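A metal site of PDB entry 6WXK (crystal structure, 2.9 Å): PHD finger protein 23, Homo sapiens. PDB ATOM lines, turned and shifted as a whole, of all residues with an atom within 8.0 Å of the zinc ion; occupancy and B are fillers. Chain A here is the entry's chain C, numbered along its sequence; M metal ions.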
ATOM      1  N   TYR A  11     -11.448 -17.145 -19.719  1.00  0.00           N
ATOM      2  CA  TYR A  11     -10.383 -16.384 -19.095  1.00  0.00           C
ATOM      3  C   TYR A  11     -10.958 -15.440 -18.038  1.00  0.00           C
ATOM      4  O   TYR A  11     -10.643 -15.547 -16.849  1.00  0.00           O
ATOM      5  CB  TYR A  11      -9.595 -15.582 -20.145  1.00  0.00           C
ATOM      6  CG  TYR A  11      -9.151 -16.340 -21.378  1.00  0.00           C
ATOM      7  CD1 TYR A  11      -8.226 -17.384 -21.315  1.00  0.00           C
ATOM      8  CD2 TYR A  11      -9.602 -15.957 -22.631  1.00  0.00           C
ATOM      9  CE1 TYR A  11      -7.818 -18.061 -22.456  1.00  0.00           C
ATOM     10  CE2 TYR A  11      -9.190 -16.614 -23.786  1.00  0.00           C
ATOM     11  CZ  TYR A  11      -8.301 -17.669 -23.697  1.00  0.00           C
ATOM     12  OH  TYR A  11      -7.900 -18.320 -24.859  1.00  0.00           O
ATOM     13  N   GLU A  23     -15.350 -23.410 -28.608  1.00  0.00           N
ATOM     14  CA  GLU A  23     -14.669 -24.519 -27.949  1.00  0.00           C
ATOM     15  C   GLU A  23     -13.198 -24.525 -28.333  1.00  0.00           C
ATOM     16  O   GLU A  23     -12.830 -24.240 -29.476  1.00  0.00           O
ATOM     17  CB  GLU A  23     -15.310 -25.833 -28.387  1.00  0.00           C
ATOM     18  CG  GLU A  23     -14.830 -27.079 -27.683  1.00  0.00           C
ATOM     19  CD  GLU A  23     -15.474 -28.338 -28.246  1.00  0.00           C
ATOM     20  OE1 GLU A  23     -16.140 -28.266 -29.297  1.00  0.00           O
ATOM     21  OE2 GLU A  23     -15.330 -29.407 -27.599  1.00  0.00           O
ATOM     22  N   CYS A  24     -12.336 -24.826 -27.356  1.00  0.00           N
ATOM     23  CA  CYS A  24     -10.925 -25.104 -27.629  1.00  0.00           C
ATOM     24  C   CYS A  24     -10.807 -26.487 -28.239  1.00  0.00           C
ATOM     25  O   CYS A  24     -11.222 -27.476 -27.624  1.00  0.00           O
ATOM     26  CB  CYS A  24     -10.097 -25.020 -26.347  1.00  0.00           C
ATOM     27  SG  CYS A  24      -8.358 -25.421 -26.587  1.00  0.00           S
ATOM     28  N   SER A  25     -10.242 -26.586 -29.437  1.00  0.00           N
ATOM     29  CA  SER A  25     -10.139 -27.894 -30.072  1.00  0.00           C
ATOM     30  C   SER A  25      -9.200 -28.844 -29.342  1.00  0.00           C
ATOM     31  O   SER A  25      -9.204 -30.042 -29.652  1.00  0.00           O
ATOM     32  CB  SER A  25      -9.719 -27.746 -31.524  1.00  0.00           C
ATOM     33  OG  SER A  25     -10.772 -27.145 -32.252  1.00  0.00           O
ATOM     34  N   LEU A  26      -8.403 -28.364 -28.389  1.00  0.00           N
ATOM     35  CA  LEU A  26      -7.428 -29.218 -27.750  1.00  0.00           C
ATOM     36  C   LEU A  26      -7.827 -29.598 -26.333  1.00  0.00           C
ATOM     37  O   LEU A  26      -7.940 -30.787 -26.024  1.00  0.00           O
ATOM     38  CB  LEU A  26      -6.055 -28.517 -27.755  1.00  0.00           C
ATOM     39  CG  LEU A  26      -4.806 -29.377 -27.533  1.00  0.00           C
ATOM     40  CD1 LEU A  26      -4.724 -30.394 -28.651  1.00  0.00           C
ATOM     41  CD2 LEU A  26      -3.555 -28.518 -27.518  1.00  0.00           C
ATOM     42  N   CYS A  27      -8.122 -28.613 -25.473  1.00  0.00           N
ATOM     43  CA  CYS A  27      -8.468 -28.897 -24.089  1.00  0.00           C
ATOM     44  C   CYS A  27      -9.969 -28.979 -23.845  1.00  0.00           C
ATOM     45  O   CYS A  27     -10.378 -29.458 -22.783  1.00  0.00           O
ATOM     46  CB  CYS A  27      -7.875 -27.844 -23.155  1.00  0.00           C
ATOM     47  SG  CYS A  27      -8.759 -26.319 -23.248  1.00  0.00           S
ATOM     48  N   GLY A  28     -10.801 -28.487 -24.771  1.00  0.00           N
ATOM     49  CA  GLY A  28     -12.242 -28.535 -24.609  1.00  0.00           C
ATOM     50  C   GLY A  28     -12.904 -27.363 -23.904  1.00  0.00           C
ATOM     51  O   GLY A  28     -14.141 -27.348 -23.812  1.00  0.00           O
ATOM     52  N   THR A  29     -12.146 -26.402 -23.384  1.00  0.00           N
ATOM     53  CA  THR A  29     -12.741 -25.308 -22.620  1.00  0.00           C
ATOM     54  C   THR A  29     -13.492 -24.359 -23.546  1.00  0.00           C
ATOM     55  O   THR A  29     -13.218 -24.267 -24.746  1.00  0.00           O
ATOM     56  CB  THR A  29     -11.671 -24.542 -21.835  1.00  0.00           C
ATOM     57  OG1 THR A  29     -12.316 -23.670 -20.903  1.00  0.00           O
ATOM     58  CG2 THR A  29     -10.817 -23.687 -22.744  1.00  0.00           C
ATOM     59  N   TRP A  30     -14.506 -23.684 -22.995  1.00  0.00           N
ATOM     60  CA  TRP A  30     -15.348 -22.742 -23.731  1.00  0.00           C
ATOM     61  C   TRP A  30     -14.900 -21.322 -23.423  1.00  0.00           C
ATOM     62  O   TRP A  30     -14.867 -20.926 -22.255  1.00  0.00           O
ATOM     63  CB  TRP A  30     -16.816 -22.936 -23.357  1.00  0.00           C
ATOM     64  CG  TRP A  30     -17.377 -24.220 -23.842  1.00  0.00           C
ATOM     65  CD1 TRP A  30     -17.533 -25.359 -23.119  1.00  0.00           C
ATOM     66  CD2 TRP A  30     -17.856 -24.501 -25.167  1.00  0.00           C
ATOM     67  NE1 TRP A  30     -18.077 -26.346 -23.918  1.00  0.00           N
ATOM     68  CE2 TRP A  30     -18.284 -25.841 -25.167  1.00  0.00           C
ATOM     69  CE3 TRP A  30     -17.965 -23.750 -26.333  1.00  0.00           C
ATOM     70  CZ2 TRP A  30     -18.813 -26.456 -26.311  1.00  0.00           C
ATOM     71  CZ3 TRP A  30     -18.486 -24.349 -27.460  1.00  0.00           C
ATOM     72  CH2 TRP A  30     -18.906 -25.687 -27.442  1.00  0.00           C
ATOM     73  N   ILE A  31     -14.588 -20.555 -24.459  1.00  0.00           N
ATOM     74  CA  ILE A  31     -14.098 -19.191 -24.324  1.00  0.00           C
ATOM     75  C   ILE A  31     -15.108 -18.227 -24.929  1.00  0.00           C
ATOM     76  O   ILE A  31     -15.574 -18.449 -26.060  1.00  0.00           O
ATOM     77  CB  ILE A  31     -12.723 -19.024 -24.984  1.00  0.00           C
ATOM     78  CG1 ILE A  31     -11.685 -19.957 -24.350  1.00  0.00           C
ATOM     79  CG2 ILE A  31     -12.277 -17.566 -24.951  1.00  0.00           C
ATOM     80  CD1 ILE A  31     -11.464 -19.691 -22.907  1.00  0.00           C
ATOM     81  N   PHE A  47     -10.170 -23.555 -33.095  1.00  0.00           N
ATOM     82  CA  PHE A  47      -9.772 -22.562 -32.127  1.00  0.00           C
ATOM     83  C   PHE A  47      -8.987 -23.202 -31.001  1.00  0.00           C
ATOM     84  O   PHE A  47      -9.307 -24.319 -30.572  1.00  0.00           O
ATOM     85  CB  PHE A  47     -10.977 -21.848 -31.545  1.00  0.00           C
ATOM     86  CG  PHE A  47     -10.642 -20.923 -30.424  1.00  0.00           C
ATOM     87  CD1 PHE A  47     -10.093 -19.670 -30.681  1.00  0.00           C
ATOM     88  CD2 PHE A  47     -10.859 -21.292 -29.106  1.00  0.00           C
ATOM     89  CE1 PHE A  47      -9.789 -18.819 -29.646  1.00  0.00           C
ATOM     90  CE2 PHE A  47     -10.555 -20.442 -28.071  1.00  0.00           C
ATOM     91  CZ  PHE A  47     -10.027 -19.205 -28.339  1.00  0.00           C
ATOM     92  N   TYR A  48      -7.987 -22.484 -30.497  1.00  0.00           N
ATOM     93  CA  TYR A  48      -7.128 -22.973 -29.431  1.00  0.00           C
ATOM     94  C   TYR A  48      -6.933 -21.880 -28.392  1.00  0.00           C
ATOM     95  O   TYR A  48      -6.593 -20.748 -28.755  1.00  0.00           O
ATOM     96  CB  TYR A  48      -5.774 -23.422 -29.997  1.00  0.00           C
ATOM     97  CG  TYR A  48      -5.923 -24.557 -30.973  1.00  0.00           C
ATOM     98  CD1 TYR A  48      -6.144 -25.859 -30.541  1.00  0.00           C
ATOM     99  CD2 TYR A  48      -5.859 -24.314 -32.334  1.00  0.00           C
ATOM    100  CE1 TYR A  48      -6.295 -26.893 -31.441  1.00  0.00           C
ATOM    101  CE2 TYR A  48      -6.008 -25.342 -33.247  1.00  0.00           C
ATOM    102  CZ  TYR A  48      -6.224 -26.629 -32.807  1.00  0.00           C
ATOM    103  OH  TYR A  48      -6.364 -27.631 -33.738  1.00  0.00           O
ATOM    104  N   CYS A  49      -7.149 -22.222 -27.132  1.00  0.00           N
ATOM    105  CA  CYS A  49      -7.084 -21.220 -26.083  1.00  0.00           C
ATOM    106  C   CYS A  49      -5.632 -20.904 -25.737  1.00  0.00           C
ATOM    107  O   CYS A  49      -4.707 -21.608 -26.162  1.00  0.00           O
ATOM    108  CB  CYS A  49      -7.849 -21.693 -24.843  1.00  0.00           C
ATOM    109  SG  CYS A  49      -7.128 -23.109 -23.956  1.00  0.00           S
ATOM    110  N   GLN A  50      -5.448 -19.817 -24.987  1.00  0.00           N
ATOM    111  CA  GLN A  50      -4.103 -19.394 -24.578  1.00  0.00           C
ATOM    112  C   GLN A  50      -3.297 -20.567 -24.038  1.00  0.00           C
ATOM    113  O   GLN A  50      -2.147 -20.780 -24.418  1.00  0.00           O
ATOM    114  CB  GLN A  50      -4.210 -18.306 -23.513  1.00  0.00           C
ATOM    115  CG  GLN A  50      -4.807 -16.971 -23.951  1.00  0.00           C
ATOM    116  CD  GLN A  50      -5.136 -16.045 -22.753  1.00  0.00           C
ATOM    117  OE1 GLN A  50      -5.003 -16.447 -21.585  1.00  0.00           O
ATOM    118  NE2 GLN A  50      -5.580 -14.828 -23.045  1.00  0.00           N
ATOM    119  N   LYS A  51      -3.912 -21.352 -23.148  1.00  0.00           N
ATOM    120  CA  LYS A  51      -3.209 -22.421 -22.459  1.00  0.00           C
ATOM    121  C   LYS A  51      -2.752 -23.510 -23.417  1.00  0.00           C
ATOM    122  O   LYS A  51      -1.777 -24.221 -23.132  1.00  0.00           O
ATOM    123  CB  LYS A  51      -4.107 -23.006 -21.368  1.00  0.00           C
ATOM    124  CG  LYS A  51      -4.381 -22.077 -20.204  1.00  0.00           C
ATOM    125  CD  LYS A  51      -5.534 -22.570 -19.357  1.00  0.00           C
ATOM    126  CE  LYS A  51      -5.211 -23.865 -18.582  1.00  0.00           C
ATOM    127  NZ  LYS A  51      -6.355 -24.266 -17.685  1.00  0.00           N
ATOM    128  N   CYS A  52      -3.442 -23.689 -24.537  1.00  0.00           N
ATOM    129  CA  CYS A  52      -3.079 -24.741 -25.483  1.00  0.00           C
ATOM    130  C   CYS A  52      -2.155 -24.252 -26.595  1.00  0.00           C
ATOM    131  O   CYS A  52      -2.212 -24.778 -27.715  1.00  0.00           O
ATOM    132  CB  CYS A  52      -4.345 -25.368 -26.052  1.00  0.00           C
ATOM    133  SG  CYS A  52      -5.239 -26.335 -24.830  1.00  0.00           S
ATOM    134  N   LYS A  53      -1.278 -23.290 -26.309  1.00  0.00           N
ATOM    135  CA  LYS A  53      -0.291 -22.843 -27.300  1.00  0.00           C
ATOM    136  C   LYS A  53       1.112 -22.717 -26.694  1.00  0.00           C
ATOM    137  O   LYS A  53       1.954 -21.980 -27.226  1.00  0.00           O
ATOM    138  CB  LYS A  53      -0.699 -21.505 -27.893  1.00  0.00           C
ATOM    139  CG  LYS A  53      -1.949 -21.559 -28.733  1.00  0.00           C
ATOM    140  CD  LYS A  53      -2.280 -20.169 -29.254  1.00  0.00           C
ATOM    141  CE  LYS A  53      -3.552 -20.169 -30.060  1.00  0.00           C
ATOM    142  NZ  LYS A  53      -3.861 -18.796 -30.545  1.00  0.00           N
HETATM  143 ZN    ZN M   1      -7.229 -25.253 -24.493  1.00  0.00          ZN
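SG of Cys 49 lies close to N of Lys 51 (3.8 Å). The side-chain sulfur (SG) of Cys 27 lies close to the backbone NH (N) of Thr 29 (3.4 Å). The backbone carbonyl oxygen (O) of Thr 29 is in hydrogen-bond range of the backbone NH (N) of Cys 24, 2.8 Å away. The backbone NH (N) of Leu 26 lies close to the side-chain sulfur (SG) of Cys 24 (3.5 Å).
Four residues have an atom within 4 Å of the zinc ion: Cys 24, Cys 27, Cys 49 and Cys 52. Along chain A the residues within 4 Å of the zinc ion span positions 24 to 52. The nearest printed residue that does not touch the zinc ion is Thr 29 (4.3 Å).
The zinc ion is bound by SG of Cys 49 (2.2 Å), SG of Cys 27 (2.2 Å), SG of Cys 52 (2.3 Å) and SG of Cys 24 (2.4 Å). The zinc ion has four donor atoms within binding distance.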
